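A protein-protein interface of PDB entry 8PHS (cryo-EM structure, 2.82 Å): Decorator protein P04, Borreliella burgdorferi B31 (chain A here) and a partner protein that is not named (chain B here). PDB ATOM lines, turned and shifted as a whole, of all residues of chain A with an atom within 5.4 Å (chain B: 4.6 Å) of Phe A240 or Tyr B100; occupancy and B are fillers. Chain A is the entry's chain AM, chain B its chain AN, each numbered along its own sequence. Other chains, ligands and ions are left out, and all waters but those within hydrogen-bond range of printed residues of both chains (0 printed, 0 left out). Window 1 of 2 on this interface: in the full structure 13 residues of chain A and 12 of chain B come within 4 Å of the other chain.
Among the printed residues, pairs that only touch across the chains: Asn A163 with Pro B117 (3.1 Å), Phe A240 with Leu B99 (3.3 Å), Gly A241 with Thr B119 (3.3 Å), Phe A240 with Thr B119 (3.6 Å), Phe A240 with Tyr B100 (3.8 Å) and Phe A240 with Ile B118 (3.9 Å).
Of the 11 printed residues of chain A, 4 touch a printed residue of chain B.
Along chain A the printed residues that touch a printed residue of chain B span positions 163 to 241.
Of the 13 printed residues of chain B, 6 touch a printed residue of chain A.
Printed residues of chain B that touch a printed residue of chain A: Arg B75, Leu B99, Tyr B100, Pro B117, Ile B118 and Thr B119.
Among the printed residues, 8 pairs touch across the chains.
Among the printed residues, Asp or Glu carboxylates within 4 Å of a Lys or Arg side-chain nitrogen of the other chain: Glu A165 with Arg B75.
OD1 of Asn A163 lies within hydrogen-bond range of OG1 of Thr B119.
NH1 of Arg B75 is in salt-bridge range of OE1 of Glu A165, at 3.3 Å.
The side-chain carboxylate (OE1) of Glu B60 sits at hydrogen-bond distance from the side-chain hydroxyl (OH) of Tyr B100, at 2.9 Å.
O of Tyr B100 sits at hydrogen-bond distance from N of Ile B118 (3.1 Å).
The side-chain amide nitrogen (ND2) of Asn A201 is in hydrogen-bond range of the backbone carbonyl oxygen (O) of Phe A240.
The backbone carbonyl oxygen of Val B73 sits at hydrogen-bond distance from the backbone NH of Tyr B100 (2.9 Å).
The backbone carbonyl oxygen of Gly A241 lies within hydrogen-bond range of the backbone NH of Asn A201 (3.2 Å).
Phe A240 touches just these residues of chain B: Leu B99 (3.3 Å), Tyr B100 (3.8 Å), Ile B118 (3.9 Å) and Thr B119 (3.6 Å).
Of the printed residues of chain A, Tyr B100 touches Phe A240.
Printed residues of chain A within 4 Å of Pro B117: Asn A163 (3.1 Å).
Of the printed residues of chain A, Thr B119 touches Asn A163 (2.7 Å), Phe A240 (3.6 Å) and Gly A241 (3.3 Å).
The nearest printed residue of chain B that does not touch Asn A163 is Glu B60 (4.2 Å).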
ATOM      1  N   ASN A 163     -33.799  16.681   0.014  1.00  0.00           N
ATOM      2  CA  ASN A 163     -33.157  16.817  -1.281  1.00  0.00           C
ATOM      3  C   ASN A 163     -34.166  17.240  -2.340  1.00  0.00           C
ATOM      4  O   ASN A 163     -35.374  17.024  -2.213  1.00  0.00           O
ATOM      5  CB  ASN A 163     -32.504  15.502  -1.696  1.00  0.00           C
ATOM      6  CG  ASN A 163     -31.583  14.963  -0.640  1.00  0.00           C
ATOM      7  OD1 ASN A 163     -31.908  13.996   0.045  1.00  0.00           O
ATOM      8  ND2 ASN A 163     -30.420  15.583  -0.499  1.00  0.00           N
ATOM      9  N   PHE A 164     -33.652  17.854  -3.399  1.00  0.00           N
ATOM     10  CA  PHE A 164     -34.474  18.246  -4.531  1.00  0.00           C
ATOM     11  C   PHE A 164     -33.670  18.073  -5.808  1.00  0.00           C
ATOM     12  O   PHE A 164     -32.463  18.318  -5.825  1.00  0.00           O
ATOM     13  CB  PHE A 164     -34.953  19.697  -4.403  1.00  0.00           C
ATOM     14  CG  PHE A 164     -35.834  20.146  -5.531  1.00  0.00           C
ATOM     15  CD1 PHE A 164     -37.122  19.657  -5.654  1.00  0.00           C
ATOM     16  CD2 PHE A 164     -35.378  21.057  -6.465  1.00  0.00           C
ATOM     17  CE1 PHE A 164     -37.938  20.068  -6.688  1.00  0.00           C
ATOM     18  CE2 PHE A 164     -36.190  21.474  -7.503  1.00  0.00           C
ATOM     19  CZ  PHE A 164     -37.471  20.977  -7.614  1.00  0.00           C
ATOM     20  N   GLU A 165     -34.344  17.644  -6.869  1.00  0.00           N
ATOM     21  CA  GLU A 165     -33.737  17.550  -8.196  1.00  0.00           C
ATOM     22  C   GLU A 165     -34.838  17.892  -9.191  1.00  0.00           C
ATOM     23  O   GLU A 165     -35.731  17.078  -9.437  1.00  0.00           O
ATOM     24  CB  GLU A 165     -33.149  16.168  -8.450  1.00  0.00           C
ATOM     25  CG  GLU A 165     -32.794  15.903  -9.901  1.00  0.00           C
ATOM     26  CD  GLU A 165     -31.811  14.760 -10.060  1.00  0.00           C
ATOM     27  OE1 GLU A 165     -31.314  14.252  -9.034  1.00  0.00           O
ATOM     28  OE2 GLU A 165     -31.534  14.369 -11.214  1.00  0.00           O
ATOM     29  N   ASN A 201     -25.804  23.901  -1.237  1.00  0.00           N
ATOM     30  CA  ASN A 201     -25.199  23.121  -2.317  1.00  0.00           C
ATOM     31  C   ASN A 201     -26.187  23.054  -3.474  1.00  0.00           C
ATOM     32  O   ASN A 201     -27.156  22.293  -3.437  1.00  0.00           O
ATOM     33  CB  ASN A 201     -24.821  21.726  -1.834  1.00  0.00           C
ATOM     34  CG  ASN A 201     -23.921  21.750  -0.618  1.00  0.00           C
ATOM     35  OD1 ASN A 201     -22.805  22.265  -0.669  1.00  0.00           O
ATOM     36  ND2 ASN A 201     -24.402  21.190   0.485  1.00  0.00           N
ATOM     37  N   ILE A 202     -25.944  23.857  -4.508  1.00  0.00           N
ATOM     38  CA  ILE A 202     -26.760  23.865  -5.717  1.00  0.00           C
ATOM     39  C   ILE A 202     -25.844  23.662  -6.915  1.00  0.00           C
ATOM     40  O   ILE A 202     -24.822  24.344  -7.042  1.00  0.00           O
ATOM     41  CB  ILE A 202     -27.560  25.173  -5.867  1.00  0.00           C
ATOM     42  CG1 ILE A 202     -28.293  25.508  -4.568  1.00  0.00           C
ATOM     43  CG2 ILE A 202     -28.544  25.063  -7.017  1.00  0.00           C
ATOM     44  CD1 ILE A 202     -29.012  26.836  -4.603  1.00  0.00           C
ATOM     45  N   TYR A 203     -26.210  22.727  -7.789  1.00  0.00           N
ATOM     46  CA  TYR A 203     -25.444  22.428  -8.990  1.00  0.00           C
ATOM     47  C   TYR A 203     -26.378  22.349 -10.187  1.00  0.00           C
ATOM     48  O   TYR A 203     -27.494  21.834 -10.081  1.00  0.00           O
ATOM     49  CB  TYR A 203     -24.669  21.116  -8.842  1.00  0.00           C
ATOM     50  CG  TYR A 203     -23.551  21.185  -7.829  1.00  0.00           C
ATOM     51  CD1 TYR A 203     -22.395  21.904  -8.094  1.00  0.00           C
ATOM     52  CD2 TYR A 203     -23.660  20.549  -6.601  1.00  0.00           C
ATOM     53  CE1 TYR A 203     -21.371  21.972  -7.170  1.00  0.00           C
ATOM     54  CE2 TYR A 203     -22.642  20.615  -5.670  1.00  0.00           C
ATOM     55  CZ  TYR A 203     -21.501  21.330  -5.960  1.00  0.00           C
ATOM     56  OH  TYR A 203     -20.483  21.400  -5.037  1.00  0.00           O
ATOM     57  N   ALA A 238     -29.873  20.408  -8.772  1.00  0.00           N
ATOM     58  CA  ALA A 238     -29.876  19.469  -7.657  1.00  0.00           C
ATOM     59  C   ALA A 238     -29.478  20.222  -6.397  1.00  0.00           C
ATOM     60  O   ALA A 238     -28.383  20.789  -6.329  1.00  0.00           O
ATOM     61  CB  ALA A 238     -28.922  18.301  -7.914  1.00  0.00           C
ATOM     62  N   ILE A 239     -30.365  20.228  -5.408  1.00  0.00           N
ATOM     63  CA  ILE A 239     -30.151  20.916  -4.141  1.00  0.00           C
ATOM     64  C   ILE A 239     -30.114  19.868  -3.041  1.00  0.00           C
ATOM     65  O   ILE A 239     -31.081  19.119  -2.856  1.00  0.00           O
ATOM     66  CB  ILE A 239     -31.248  21.955  -3.864  1.00  0.00           C
ATOM     67  CG1 ILE A 239     -31.331  22.963  -5.010  1.00  0.00           C
ATOM     68  CG2 ILE A 239     -30.993  22.656  -2.541  1.00  0.00           C
ATOM     69  CD1 ILE A 239     -32.324  24.074  -4.769  1.00  0.00           C
ATOM     70  N   PHE A 240     -29.001  19.815  -2.310  1.00  0.00           N
ATOM     71  CA  PHE A 240     -28.817  18.856  -1.220  1.00  0.00           C
ATOM     72  C   PHE A 240     -28.201  19.561  -0.010  1.00  0.00           C
ATOM     73  O   PHE A 240     -26.981  19.638   0.145  1.00  0.00           O
ATOM     74  CB  PHE A 240     -27.995  17.644  -1.701  1.00  0.00           C
ATOM     75  CG  PHE A 240     -26.638  17.986  -2.263  1.00  0.00           C
ATOM     76  CD1 PHE A 240     -26.509  18.413  -3.574  1.00  0.00           C
ATOM     77  CD2 PHE A 240     -25.489  17.812  -1.509  1.00  0.00           C
ATOM     78  CE1 PHE A 240     -25.271  18.712  -4.104  1.00  0.00           C
ATOM     79  CE2 PHE A 240     -24.247  18.110  -2.034  1.00  0.00           C
ATOM     80  CZ  PHE A 240     -24.138  18.557  -3.333  1.00  0.00           C
ATOM     81  N   GLY A 241     -29.064  20.096   0.847  1.00  0.00           N
ATOM     82  CA  GLY A 241     -28.647  20.584   2.148  1.00  0.00           C
ATOM     83  C   GLY A 241     -27.814  21.853   2.091  1.00  0.00           C
ATOM     84  O   GLY A 241     -27.570  22.445   1.042  1.00  0.00           O
ATOM     85  N   ASN A 242     -27.365  22.262   3.272  1.00  0.00           N
ATOM     86  CA  ASN A 242     -26.559  23.460   3.439  1.00  0.00           C
ATOM     87  C   ASN A 242     -25.078  23.144   3.268  1.00  0.00           C
ATOM     88  O   ASN A 242     -24.642  21.995   3.378  1.00  0.00           O
ATOM     89  CB  ASN A 242     -26.802  24.083   4.814  1.00  0.00           C
ATOM     90  CG  ASN A 242     -26.572  23.101   5.949  1.00  0.00           C
ATOM     91  OD1 ASN A 242     -25.453  22.643   6.175  1.00  0.00           O
ATOM     92  ND2 ASN A 242     -27.637  22.774   6.671  1.00  0.00           N
ATOM     93  N   GLU B  60     -31.315   6.501  -3.087  1.00  0.00           N
ATOM     94  CA  GLU B  60     -31.233   6.844  -4.502  1.00  0.00           C
ATOM     95  C   GLU B  60     -30.229   5.935  -5.190  1.00  0.00           C
ATOM     96  O   GLU B  60     -29.123   5.737  -4.683  1.00  0.00           O
ATOM     97  CB  GLU B  60     -30.829   8.309  -4.689  1.00  0.00           C
ATOM     98  CG  GLU B  60     -31.720   9.292  -3.957  1.00  0.00           C
ATOM     99  CD  GLU B  60     -31.165  10.701  -3.963  1.00  0.00           C
ATOM    100  OE1 GLU B  60     -30.058  10.903  -4.506  1.00  0.00           O
ATOM    101  OE2 GLU B  60     -31.835  11.605  -3.426  1.00  0.00           O
ATOM    102  N   HIS B  62     -27.647   5.290  -8.238  1.00  0.00           N
ATOM    103  CA  HIS B  62     -26.848   6.099  -9.143  1.00  0.00           C
ATOM    104  C   HIS B  62     -25.799   5.249  -9.845  1.00  0.00           C
ATOM    105  O   HIS B  62     -25.274   4.295  -9.251  1.00  0.00           O
ATOM    106  CB  HIS B  62     -26.154   7.244  -8.393  1.00  0.00           C
ATOM    107  CG  HIS B  62     -27.055   8.396  -8.073  1.00  0.00           C
ATOM    108  ND1 HIS B  62     -27.429   8.710  -6.785  1.00  0.00           N
ATOM    109  CD2 HIS B  62     -27.644   9.317  -8.871  1.00  0.00           C
ATOM    110  CE1 HIS B  62     -28.219   9.769  -6.803  1.00  0.00           C
ATOM    111  NE2 HIS B  62     -28.364  10.157  -8.058  1.00  0.00           N
ATOM    112  N   VAL B  73     -19.514   9.536  -1.209  1.00  0.00           N
ATOM    113  CA  VAL B  73     -19.614   9.623  -2.659  1.00  0.00           C
ATOM    114  C   VAL B  73     -19.917  11.060  -3.055  1.00  0.00           C
ATOM    115  O   VAL B  73     -20.701  11.753  -2.393  1.00  0.00           O
ATOM    116  CB  VAL B  73     -20.689   8.666  -3.216  1.00  0.00           C
ATOM    117  CG1 VAL B  73     -20.279   7.225  -2.986  1.00  0.00           C
ATOM    118  CG2 VAL B  73     -22.038   8.942  -2.575  1.00  0.00           C
ATOM    119  N   LYS B  74     -19.282  11.497  -4.141  1.00  0.00           N
ATOM    120  CA  LYS B  74     -19.498  12.796  -4.751  1.00  0.00           C
ATOM    121  C   LYS B  74     -20.038  12.599  -6.160  1.00  0.00           C
ATOM    122  O   LYS B  74     -19.701  11.623  -6.842  1.00  0.00           O
ATOM    123  CB  LYS B  74     -18.204  13.612  -4.820  1.00  0.00           C
ATOM    124  CG  LYS B  74     -17.066  12.901  -5.531  1.00  0.00           C
ATOM    125  CD  LYS B  74     -15.798  13.735  -5.520  1.00  0.00           C
ATOM    126  CE  LYS B  74     -14.621  12.957  -6.085  1.00  0.00           C
ATOM    127  NZ  LYS B  74     -13.342  13.708  -5.962  1.00  0.00           N
ATOM    128  N   ARG B  75     -20.875  13.540  -6.590  1.00  0.00           N
ATOM    129  CA  ARG B  75     -21.518  13.479  -7.897  1.00  0.00           C
ATOM    130  C   ARG B  75     -20.650  14.210  -8.914  1.00  0.00           C
ATOM    131  O   ARG B  75     -20.466  15.428  -8.825  1.00  0.00           O
ATOM    132  CB  ARG B  75     -22.918  14.081  -7.833  1.00  0.00           C
ATOM    133  CG  ARG B  75     -23.786  13.739  -9.028  1.00  0.00           C
ATOM    134  CD  ARG B  75     -25.262  13.876  -8.702  1.00  0.00           C
ATOM    135  NE  ARG B  75     -26.100  13.416  -9.802  1.00  0.00           N
ATOM    136  CZ  ARG B  75     -27.423  13.352  -9.758  1.00  0.00           C
ATOM    137  NH1 ARG B  75     -28.098  13.708  -8.677  1.00  0.00           N
ATOM    138  NH2 ARG B  75     -28.087  12.922 -10.828  1.00  0.00           N
ATOM    139  N   ASP B  98     -17.211  18.634  -1.864  1.00  0.00           N
ATOM    140  CA  ASP B  98     -17.927  17.949  -2.928  1.00  0.00           C
ATOM    141  C   ASP B  98     -18.752  16.774  -2.423  1.00  0.00           C
ATOM    142  O   ASP B  98     -19.356  16.070  -3.237  1.00  0.00           O
ATOM    143  CB  ASP B  98     -16.944  17.461  -3.995  1.00  0.00           C
ATOM    144  CG  ASP B  98     -16.096  18.580  -4.562  1.00  0.00           C
ATOM    145  OD1 ASP B  98     -16.267  19.737  -4.124  1.00  0.00           O
ATOM    146  OD2 ASP B  98     -15.260  18.304  -5.447  1.00  0.00           O
ATOM    147  N   LEU B  99     -18.792  16.547  -1.113  1.00  0.00           N
ATOM    148  CA  LEU B  99     -19.510  15.401  -0.573  1.00  0.00           C
ATOM    149  C   LEU B  99     -20.988  15.476  -0.924  1.00  0.00           C
ATOM    150  O   LEU B  99     -21.641  16.501  -0.709  1.00  0.00           O
ATOM    151  CB  LEU B  99     -19.333  15.335   0.944  1.00  0.00           C
ATOM    152  CG  LEU B  99     -20.028  14.164   1.638  1.00  0.00           C
ATOM    153  CD1 LEU B  99     -19.402  12.843   1.225  1.00  0.00           C
ATOM    154  CD2 LEU B  99     -19.984  14.335   3.145  1.00  0.00           C
ATOM    155  N   TYR B 100     -21.513  14.384  -1.470  1.00  0.00           N
ATOM    156  CA  TYR B 100     -22.918  14.289  -1.842  1.00  0.00           C
ATOM    157  C   TYR B 100     -23.691  13.285  -1.008  1.00  0.00           C
ATOM    158  O   TYR B 100     -24.853  13.530  -0.676  1.00  0.00           O
ATOM    159  CB  TYR B 100     -23.051  13.918  -3.323  1.00  0.00           C
ATOM    160  CG  TYR B 100     -24.479  13.727  -3.777  1.00  0.00           C
ATOM    161  CD1 TYR B 100     -25.349  14.805  -3.861  1.00  0.00           C
ATOM    162  CD2 TYR B 100     -24.962  12.471  -4.108  1.00  0.00           C
ATOM    163  CE1 TYR B 100     -26.655  14.638  -4.271  1.00  0.00           C
ATOM    164  CE2 TYR B 100     -26.268  12.293  -4.519  1.00  0.00           C
ATOM    165  CZ  TYR B 100     -27.110  13.381  -4.598  1.00  0.00           C
ATOM    166  OH  TYR B 100     -28.412  13.212  -5.007  1.00  0.00           O
ATOM    167  N   GLY B 101     -23.080  12.163  -0.655  1.00  0.00           N
ATOM    168  CA  GLY B 101     -23.786  11.181   0.139  1.00  0.00           C
ATOM    169  C   GLY B 101     -22.883  10.060   0.594  1.00  0.00           C
ATOM    170  O   GLY B 101     -21.659  10.177   0.561  1.00  0.00           O
ATOM    171  N   ILE B 115     -27.444   5.028  -2.507  1.00  0.00           N
ATOM    172  CA  ILE B 115     -26.836   6.172  -1.847  1.00  0.00           C
ATOM    173  C   ILE B 115     -27.857   6.800  -0.915  1.00  0.00           C
ATOM    174  O   ILE B 115     -29.019   6.994  -1.295  1.00  0.00           O
ATOM    175  CB  ILE B 115     -26.328   7.204  -2.872  1.00  0.00           C
ATOM    176  CG1 ILE B 115     -25.197   6.601  -3.704  1.00  0.00           C
ATOM    177  CG2 ILE B 115     -25.868   8.473  -2.179  1.00  0.00           C
ATOM    178  CD1 ILE B 115     -24.669   7.525  -4.760  1.00  0.00           C
ATOM    179  N   PRO B 117     -28.510  10.292   0.775  1.00  0.00           N
ATOM    180  CA  PRO B 117     -28.024  11.665   0.612  1.00  0.00           C
ATOM    181  C   PRO B 117     -27.563  12.254   1.936  1.00  0.00           C
ATOM    182  O   PRO B 117     -27.949  11.811   3.018  1.00  0.00           O
ATOM    183  CB  PRO B 117     -29.244  12.414   0.065  1.00  0.00           C
ATOM    184  CG  PRO B 117     -30.150  11.346  -0.465  1.00  0.00           C
ATOM    185  CD  PRO B 117     -29.930  10.164   0.417  1.00  0.00           C
ATOM    186  N   ILE B 118     -26.711  13.277   1.826  1.00  0.00           N
ATOM    187  CA  ILE B 118     -26.110  13.883   3.011  1.00  0.00           C
ATOM    188  C   ILE B 118     -27.171  14.513   3.903  1.00  0.00           C
ATOM    189  O   ILE B 118     -26.963  14.674   5.112  1.00  0.00           O
ATOM    190  CB  ILE B 118     -25.033  14.905   2.595  1.00  0.00           C
ATOM    191  CG1 ILE B 118     -24.162  15.281   3.795  1.00  0.00           C
ATOM    192  CG2 ILE B 118     -25.670  16.142   1.981  1.00  0.00           C
ATOM    193  CD1 ILE B 118     -23.564  14.090   4.504  1.00  0.00           C
ATOM    194  N   THR B 119     -28.324  14.866   3.338  1.00  0.00           N
ATOM    195  CA  THR B 119     -29.414  15.449   4.109  1.00  0.00           C
ATOM    196  C   THR B 119     -30.168  14.424   4.944  1.00  0.00           C
ATOM    197  O   THR B 119     -31.100  14.802   5.662  1.00  0.00           O
ATOM    198  CB  THR B 119     -30.395  16.161   3.177  1.00  0.00           C
ATOM    199  OG1 THR B 119     -31.069  15.194   2.364  1.00  0.00           O
ATOM    200  CG2 THR B 119     -29.657  17.135   2.282  1.00  0.00           C
